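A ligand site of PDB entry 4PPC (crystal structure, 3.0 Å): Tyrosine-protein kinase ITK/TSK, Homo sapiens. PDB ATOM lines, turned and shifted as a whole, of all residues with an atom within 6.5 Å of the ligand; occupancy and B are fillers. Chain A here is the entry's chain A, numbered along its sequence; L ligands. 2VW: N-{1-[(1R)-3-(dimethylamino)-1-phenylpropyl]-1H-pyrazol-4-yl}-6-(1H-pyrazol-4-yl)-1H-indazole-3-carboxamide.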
ATOM      1  N   VAL A  34       7.017   4.110   9.423  1.00  0.00           N
ATOM      2  CA  VAL A  34       8.029   4.864   8.690  1.00  0.00           C
ATOM      3  C   VAL A  34       9.452   4.430   9.049  1.00  0.00           C
ATOM      4  O   VAL A  34       9.672   3.850  10.115  1.00  0.00           O
ATOM      5  CB  VAL A  34       7.886   6.398   8.888  1.00  0.00           C
ATOM      6  CG1 VAL A  34       6.689   6.986   8.138  1.00  0.00           C
ATOM      7  CG2 VAL A  34       7.847   6.783  10.375  1.00  0.00           C
ATOM      8  N   ALA A  35      10.417   4.781   8.181  1.00  0.00           N
ATOM      9  CA  ALA A  35      11.835   4.535   8.423  1.00  0.00           C
ATOM     10  C   ALA A  35      12.502   5.878   8.724  1.00  0.00           C
ATOM     11  O   ALA A  35      12.484   6.775   7.881  1.00  0.00           O
ATOM     12  CB  ALA A  35      12.475   3.882   7.207  1.00  0.00           C
ATOM     13  N   LYS A  37      15.786   8.044   9.504  1.00  0.00           N
ATOM     14  CA  LYS A  37      17.251   8.137   9.407  1.00  0.00           C
ATOM     15  C   LYS A  37      17.729   9.288  10.290  1.00  0.00           C
ATOM     16  O   LYS A  37      17.270  10.418  10.129  1.00  0.00           O
ATOM     17  CB  LYS A  37      17.734   8.293   7.957  1.00  0.00           C
ATOM     18  CG  LYS A  37      19.213   7.959   7.793  1.00  0.00           C
ATOM     19  CD  LYS A  37      19.792   8.423   6.458  1.00  0.00           C
ATOM     20  CE  LYS A  37      20.302   7.292   5.597  1.00  0.00           C
ATOM     21  NZ  LYS A  37      21.508   6.629   6.168  1.00  0.00           N
ATOM     22  N   VAL A  65      12.084   5.573  -2.684  1.00  0.00           N
ATOM     23  CA  VAL A  65      11.642   5.663  -1.284  1.00  0.00           C
ATOM     24  C   VAL A  65      11.441   7.135  -0.936  1.00  0.00           C
ATOM     25  O   VAL A  65      12.388   7.920  -0.897  1.00  0.00           O
ATOM     26  CB  VAL A  65      12.572   4.898  -0.312  1.00  0.00           C
ATOM     27  CG1 VAL A  65      12.258   5.221   1.152  1.00  0.00           C
ATOM     28  CG2 VAL A  65      12.475   3.395  -0.548  1.00  0.00           C
ATOM     29  N   PHE A  81      11.416   8.771   6.251  1.00  0.00           N
ATOM     30  CA  PHE A  81      11.253   8.064   4.969  1.00  0.00           C
ATOM     31  C   PHE A  81      10.123   7.050   4.960  1.00  0.00           C
ATOM     32  O   PHE A  81       9.640   6.624   6.012  1.00  0.00           O
ATOM     33  CB  PHE A  81      12.558   7.376   4.553  1.00  0.00           C
ATOM     34  CG  PHE A  81      13.659   8.311   4.138  1.00  0.00           C
ATOM     35  CD1 PHE A  81      14.704   8.588   5.007  1.00  0.00           C
ATOM     36  CD2 PHE A  81      13.669   8.881   2.876  1.00  0.00           C
ATOM     37  CE1 PHE A  81      15.750   9.438   4.612  1.00  0.00           C
ATOM     38  CE2 PHE A  81      14.704   9.736   2.488  1.00  0.00           C
ATOM     39  CZ  PHE A  81      15.725  10.013   3.364  1.00  0.00           C
ATOM     40  N   GLU A  82       9.726   6.635   3.746  1.00  0.00           N
ATOM     41  CA  GLU A  82       8.701   5.642   3.439  1.00  0.00           C
ATOM     42  C   GLU A  82       9.131   4.275   4.002  1.00  0.00           C
ATOM     43  O   GLU A  82      10.311   3.956   3.970  1.00  0.00           O
ATOM     44  CB  GLU A  82       8.525   5.559   1.918  1.00  0.00           C
ATOM     45  CG  GLU A  82       7.302   4.804   1.418  1.00  0.00           C
ATOM     46  CD  GLU A  82       7.254   4.600  -0.084  1.00  0.00           C
ATOM     47  OE1 GLU A  82       6.744   3.534  -0.513  1.00  0.00           O
ATOM     48  OE2 GLU A  82       7.718   5.482  -0.838  1.00  0.00           O
ATOM     49  N   PHE A  83       8.170   3.490   4.533  1.00  0.00           N
ATOM     50  CA  PHE A  83       8.468   2.157   5.065  1.00  0.00           C
ATOM     51  C   PHE A  83       8.226   1.074   4.021  1.00  0.00           C
ATOM     52  O   PHE A  83       7.143   0.998   3.443  1.00  0.00           O
ATOM     53  CB  PHE A  83       7.687   1.859   6.349  1.00  0.00           C
ATOM     54  CG  PHE A  83       8.035   0.535   6.992  1.00  0.00           C
ATOM     55  CD1 PHE A  83       9.223   0.377   7.705  1.00  0.00           C
ATOM     56  CD2 PHE A  83       7.163  -0.545   6.908  1.00  0.00           C
ATOM     57  CE1 PHE A  83       9.545  -0.851   8.280  1.00  0.00           C
ATOM     58  CE2 PHE A  83       7.482  -1.768   7.503  1.00  0.00           C
ATOM     59  CZ  PHE A  83       8.667  -1.918   8.193  1.00  0.00           C
ATOM     60  N   MET A  84       9.255   0.232   3.811  1.00  0.00           N
ATOM     61  CA  MET A  84       9.199  -0.872   2.866  1.00  0.00           C
ATOM     62  C   MET A  84       9.087  -2.161   3.660  1.00  0.00           C
ATOM     63  O   MET A  84       9.976  -2.489   4.432  1.00  0.00           O
ATOM     64  CB  MET A  84      10.427  -0.846   1.941  1.00  0.00           C
ATOM     65  CG  MET A  84      10.580   0.464   1.181  1.00  0.00           C
ATOM     66  SD  MET A  84       9.226   0.783   0.007  1.00  0.00           S
ATOM     67  CE  MET A  84       9.682  -0.336  -1.312  1.00  0.00           C
ATOM     68  N   GLU A  85       7.936  -2.833   3.507  1.00  0.00           N
ATOM     69  CA  GLU A  85       7.511  -4.036   4.237  1.00  0.00           C
ATOM     70  C   GLU A  85       8.488  -5.213   4.302  1.00  0.00           C
ATOM     71  O   GLU A  85       8.483  -5.923   5.316  1.00  0.00           O
ATOM     72  CB  GLU A  85       6.170  -4.540   3.680  1.00  0.00           C
ATOM     73  CG  GLU A  85       4.955  -3.732   4.115  1.00  0.00           C
ATOM     74  CD  GLU A  85       4.640  -3.720   5.597  1.00  0.00           C
ATOM     75  OE1 GLU A  85       4.482  -4.819   6.183  1.00  0.00           O
ATOM     76  OE2 GLU A  85       4.540  -2.617   6.171  1.00  0.00           O
ATOM     77  N   HIS A  86       9.304  -5.440   3.259  1.00  0.00           N
ATOM     78  CA  HIS A  86      10.196  -6.606   3.202  1.00  0.00           C
ATOM     79  C   HIS A  86      11.710  -6.298   3.283  1.00  0.00           C
ATOM     80  O   HIS A  86      12.529  -7.170   3.001  1.00  0.00           O
ATOM     81  CB  HIS A  86       9.873  -7.462   1.967  1.00  0.00           C
ATOM     82  CG  HIS A  86       8.418  -7.790   1.838  1.00  0.00           C
ATOM     83  ND1 HIS A  86       7.802  -8.694   2.696  1.00  0.00           N
ATOM     84  CD2 HIS A  86       7.495  -7.299   0.992  1.00  0.00           C
ATOM     85  CE1 HIS A  86       6.537  -8.733   2.326  1.00  0.00           C
ATOM     86  NE2 HIS A  86       6.301  -7.914   1.297  1.00  0.00           N
ATOM     87  N   GLY A  87      12.058  -5.075   3.700  1.00  0.00           N
ATOM     88  CA  GLY A  87      13.437  -4.647   3.876  1.00  0.00           C
ATOM     89  C   GLY A  87      14.286  -4.607   2.622  1.00  0.00           C
ATOM     90  O   GLY A  87      13.750  -4.521   1.509  1.00  0.00           O
ATOM     91  N   CYS A  88      15.629  -4.673   2.799  1.00  0.00           N
ATOM     92  CA  CYS A  88      16.591  -4.608   1.694  1.00  0.00           C
ATOM     93  C   CYS A  88      16.589  -5.864   0.804  1.00  0.00           C
ATOM     94  O   CYS A  88      16.398  -6.979   1.284  1.00  0.00           O
ATOM     95  CB  CYS A  88      18.002  -4.271   2.177  1.00  0.00           C
ATOM     96  SG  CYS A  88      18.882  -5.640   2.976  1.00  0.00           S
ATOM     97  N   ASP A  91      19.353  -9.025   1.249  1.00  0.00           N
ATOM     98  CA  ASP A  91      18.940 -10.080   2.176  1.00  0.00           C
ATOM     99  C   ASP A  91      17.725 -10.847   1.628  1.00  0.00           C
ATOM    100  O   ASP A  91      17.656 -12.072   1.780  1.00  0.00           O
ATOM    101  CB  ASP A  91      18.622  -9.498   3.569  1.00  0.00           C
ATOM    102  CG  ASP A  91      19.789  -8.837   4.290  1.00  0.00           C
ATOM    103  OD1 ASP A  91      20.937  -8.946   3.808  1.00  0.00           O
ATOM    104  OD2 ASP A  91      19.550  -8.209   5.343  1.00  0.00           O
ATOM    105  N   TYR A  92      16.789 -10.127   0.967  1.00  0.00           N
ATOM    106  CA  TYR A  92      15.564 -10.652   0.351  1.00  0.00           C
ATOM    107  C   TYR A  92      15.860 -11.740  -0.681  1.00  0.00           C
ATOM    108  O   TYR A  92      15.114 -12.706  -0.769  1.00  0.00           O
ATOM    109  CB  TYR A  92      14.746  -9.515  -0.269  1.00  0.00           C
ATOM    110  CG  TYR A  92      13.372  -9.930  -0.749  1.00  0.00           C
ATOM    111  CD1 TYR A  92      12.294  -9.999   0.128  1.00  0.00           C
ATOM    112  CD2 TYR A  92      13.135 -10.200  -2.103  1.00  0.00           C
ATOM    113  CE1 TYR A  92      11.026 -10.361  -0.313  1.00  0.00           C
ATOM    114  CE2 TYR A  92      11.861 -10.550  -2.548  1.00  0.00           C
ATOM    115  CZ  TYR A  92      10.814 -10.638  -1.650  1.00  0.00           C
ATOM    116  OH  TYR A  92       9.564 -11.006  -2.087  1.00  0.00           O
ATOM    117  N   THR A  95      17.609 -14.901   1.345  1.00  0.00           N
ATOM    118  CA  THR A  95      16.579 -15.562   2.147  1.00  0.00           C
ATOM    119  C   THR A  95      15.634 -16.404   1.288  1.00  0.00           C
ATOM    120  O   THR A  95      15.379 -17.562   1.622  1.00  0.00           O
ATOM    121  CB  THR A  95      15.848 -14.530   3.022  1.00  0.00           C
ATOM    122  OG1 THR A  95      16.759 -14.004   3.978  1.00  0.00           O
ATOM    123  CG2 THR A  95      14.622 -15.100   3.727  1.00  0.00           C
ATOM    124  N   ASN A 133      20.859  -1.032  -0.681  1.00  0.00           N
ATOM    125  CA  ASN A 133      20.181   0.275  -0.723  1.00  0.00           C
ATOM    126  C   ASN A 133      18.908   0.255  -1.598  1.00  0.00           C
ATOM    127  O   ASN A 133      18.337   1.310  -1.886  1.00  0.00           O
ATOM    128  CB  ASN A 133      21.158   1.371  -1.166  1.00  0.00           C
ATOM    129  CG  ASN A 133      22.294   1.577  -0.191  1.00  0.00           C
ATOM    130  OD1 ASN A 133      22.098   1.905   0.980  1.00  0.00           O
ATOM    131  ND2 ASN A 133      23.521   1.384  -0.671  1.00  0.00           N
ATOM    132  N   LEU A 135      15.076  -1.468  -1.721  1.00  0.00           N
ATOM    133  CA  LEU A 135      14.122  -2.060  -0.786  1.00  0.00           C
ATOM    134  C   LEU A 135      12.889  -2.676  -1.445  1.00  0.00           C
ATOM    135  O   LEU A 135      12.382  -2.148  -2.434  1.00  0.00           O
ATOM    136  CB  LEU A 135      13.709  -1.042   0.273  1.00  0.00           C
ATOM    137  CG  LEU A 135      14.826  -0.458   1.137  1.00  0.00           C
ATOM    138  CD1 LEU A 135      14.604   0.991   1.361  1.00  0.00           C
ATOM    139  CD2 LEU A 135      14.943  -1.185   2.457  1.00  0.00           C
ATOM    140  N   VAL A 136      12.400  -3.778  -0.843  1.00  0.00           N
ATOM    141  CA  VAL A 136      11.251  -4.562  -1.282  1.00  0.00           C
ATOM    142  C   VAL A 136       9.979  -4.172  -0.491  1.00  0.00           C
ATOM    143  O   VAL A 136       9.985  -4.203   0.735  1.00  0.00           O
ATOM    144  CB  VAL A 136      11.532  -6.093  -1.207  1.00  0.00           C
ATOM    145  CG1 VAL A 136      10.452  -6.904  -1.919  1.00  0.00           C
ATOM    146  CG2 VAL A 136      12.917  -6.422  -1.763  1.00  0.00           C
ATOM    147  N   SER A 145      16.767   3.712  -2.573  1.00  0.00           N
ATOM    148  CA  SER A 145      16.916   4.561  -1.388  1.00  0.00           C
ATOM    149  C   SER A 145      18.369   4.992  -1.158  1.00  0.00           C
ATOM    150  O   SER A 145      19.274   4.424  -1.765  1.00  0.00           O
ATOM    151  CB  SER A 145      16.383   3.837  -0.151  1.00  0.00           C
ATOM    152  OG  SER A 145      17.201   2.713   0.145  1.00  0.00           O
ATOM    153  N   ASP A 146      18.589   5.974  -0.251  1.00  0.00           N
ATOM    154  CA  ASP A 146      19.886   6.538   0.171  1.00  0.00           C
ATOM    155  C   ASP A 146      20.580   7.364  -0.925  1.00  0.00           C
ATOM    156  O   ASP A 146      21.627   6.963  -1.441  1.00  0.00           O
ATOM    157  CB  ASP A 146      20.829   5.458   0.759  1.00  0.00           C
ATOM    158  CG  ASP A 146      21.208   5.668   2.204  1.00  0.00           C
ATOM    159  OD1 ASP A 146      21.679   6.778   2.543  1.00  0.00           O
ATOM    160  OD2 ASP A 146      21.084   4.697   2.996  1.00  0.00           O
ATOM    161  N   PHE A 147      20.010   8.533  -1.239  1.00  0.00           N
ATOM    162  CA  PHE A 147      20.530   9.447  -2.261  1.00  0.00           C
ATOM    163  C   PHE A 147      20.261  10.911  -1.914  1.00  0.00           C
ATOM    164  O   PHE A 147      20.845  11.449  -0.976  1.00  0.00           O
ATOM    165  CB  PHE A 147      19.962   9.100  -3.655  1.00  0.00           C
ATOM    166  CG  PHE A 147      18.463   8.920  -3.711  1.00  0.00           C
ATOM    167  CD1 PHE A 147      17.618  10.005  -3.908  1.00  0.00           C
ATOM    168  CD2 PHE A 147      17.890   7.665  -3.578  1.00  0.00           C
ATOM    169  CE1 PHE A 147      16.234   9.847  -3.959  1.00  0.00           C
ATOM    170  CE2 PHE A 147      16.502   7.499  -3.627  1.00  0.00           C
ATOM    171  CZ  PHE A 147      15.688   8.584  -3.819  1.00  0.00           C
HETATM  172  C1  2VW L   1      11.822  -9.157   6.440  1.00  0.00           C
HETATM  173  N2  2VW L   1      13.257  -9.028   6.767  1.00  0.00           N
HETATM  174  C3  2VW L   1      14.038  -8.475   5.654  1.00  0.00           C
HETATM  175  C4  2VW L   1      13.609  -8.400   8.059  1.00  0.00           C
HETATM  176  C5  2VW L   1      12.621  -7.318   8.513  1.00  0.00           C
HETATM  177  C6  2VW L   1      13.308  -5.962   8.668  1.00  0.00           C
HETATM  178  C8  2VW L   1      13.279  -5.563  10.133  1.00  0.00           C
HETATM  179  C9  2VW L   1      14.451  -5.710  10.882  1.00  0.00           C
HETATM  180  C10 2VW L   1      14.445  -5.392  12.234  1.00  0.00           C
HETATM  181  C11 2VW L   1      13.278  -4.932  12.830  1.00  0.00           C
HETATM  182  C12 2VW L   1      12.104  -4.783  12.091  1.00  0.00           C
HETATM  183  C13 2VW L   1      12.106  -5.111  10.740  1.00  0.00           C
HETATM  184  N14 2VW L   1      12.628  -4.941   7.859  1.00  0.00           N
HETATM  185  C15 2VW L   1      13.118  -3.704   7.559  1.00  0.00           C
HETATM  186  C16 2VW L   1      12.176  -3.059   6.820  1.00  0.00           C
HETATM  187  C17 2VW L   1      11.081  -3.932   6.692  1.00  0.00           C
HETATM  188  N18 2VW L   1      11.343  -5.043   7.313  1.00  0.00           N
HETATM  189  N19 2VW L   1      12.220  -1.775   6.244  1.00  0.00           N
HETATM  190  C20 2VW L   1      13.332  -1.055   5.932  1.00  0.00           C
HETATM  191  O21 2VW L   1      14.462  -1.466   6.151  1.00  0.00           O
HETATM  192  C22 2VW L   1      13.163   0.270   5.309  1.00  0.00           C
HETATM  193  C23 2VW L   1      14.199   1.271   5.024  1.00  0.00           C
HETATM  194  C24 2VW L   1      15.589   1.351   5.208  1.00  0.00           C
HETATM  195  C25 2VW L   1      16.268   2.474   4.780  1.00  0.00           C
HETATM  196  C26 2VW L   1      15.579   3.553   4.174  1.00  0.00           C
HETATM  197  C27 2VW L   1      14.187   3.476   4.000  1.00  0.00           C
HETATM  198  C28 2VW L   1      13.495   2.333   4.409  1.00  0.00           C
HETATM  199  N29 2VW L   1      12.186   1.954   4.370  1.00  0.00           N
HETATM  200  N31 2VW L   1      12.022   0.780   4.879  1.00  0.00           N
HETATM  201  C32 2VW L   1      16.326   4.767   3.727  1.00  0.00           C
HETATM  202  C33 2VW L   1      17.655   5.021   3.913  1.00  0.00           C
HETATM  203  N34 2VW L   1      17.927   6.223   3.354  1.00  0.00           N
HETATM  204  N36 2VW L   1      16.748   6.730   2.813  1.00  0.00           N
HETATM  205  C37 2VW L   1      15.786   5.860   3.019  1.00  0.00           C
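The backbone NH (N) of Met 84 sits at hydrogen-bond distance from a nitrogen (N31) of the ligand (3.0 Å). N19 of the ligand sits close to O of Met 84, 3.0 Å away. N29 of the ligand is in hydrogen-bond range of O of Glu 82, at 2.8 Å.
O of Gly 87 sits at hydrogen-bond distance from N of Val 136, at 2.8 Å. The backbone carbonyl oxygen (O) of Ala 35 lies within hydrogen-bond range of the backbone NH (N) of Phe 81 (2.8 Å). O of Asn 133 lies within hydrogen-bond range of OG of Ser 145, 2.7 Å away. The backbone NH (N) of His 86 is in hydrogen-bond range of the backbone carbonyl oxygen (O) of Val 136, 2.9 Å away. NZ of Lys 37 lies within salt-bridge range of OD1 of Asp 146, at 3.6 Å.
Residues that only touch the ligand: Ala 35 (3.4 Å), Lys 37 (3.4 Å), Val 65 (3.9 Å), Phe 81 (3.4 Å), Phe 83 (3.5 Å), Glu 85 (3.6 Å), His 86 (3.3 Å), Gly 87 (3.3 Å), Leu 135 (3.5 Å), Ser 145 (3.8 Å) and Asp 146 (3.5 Å).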
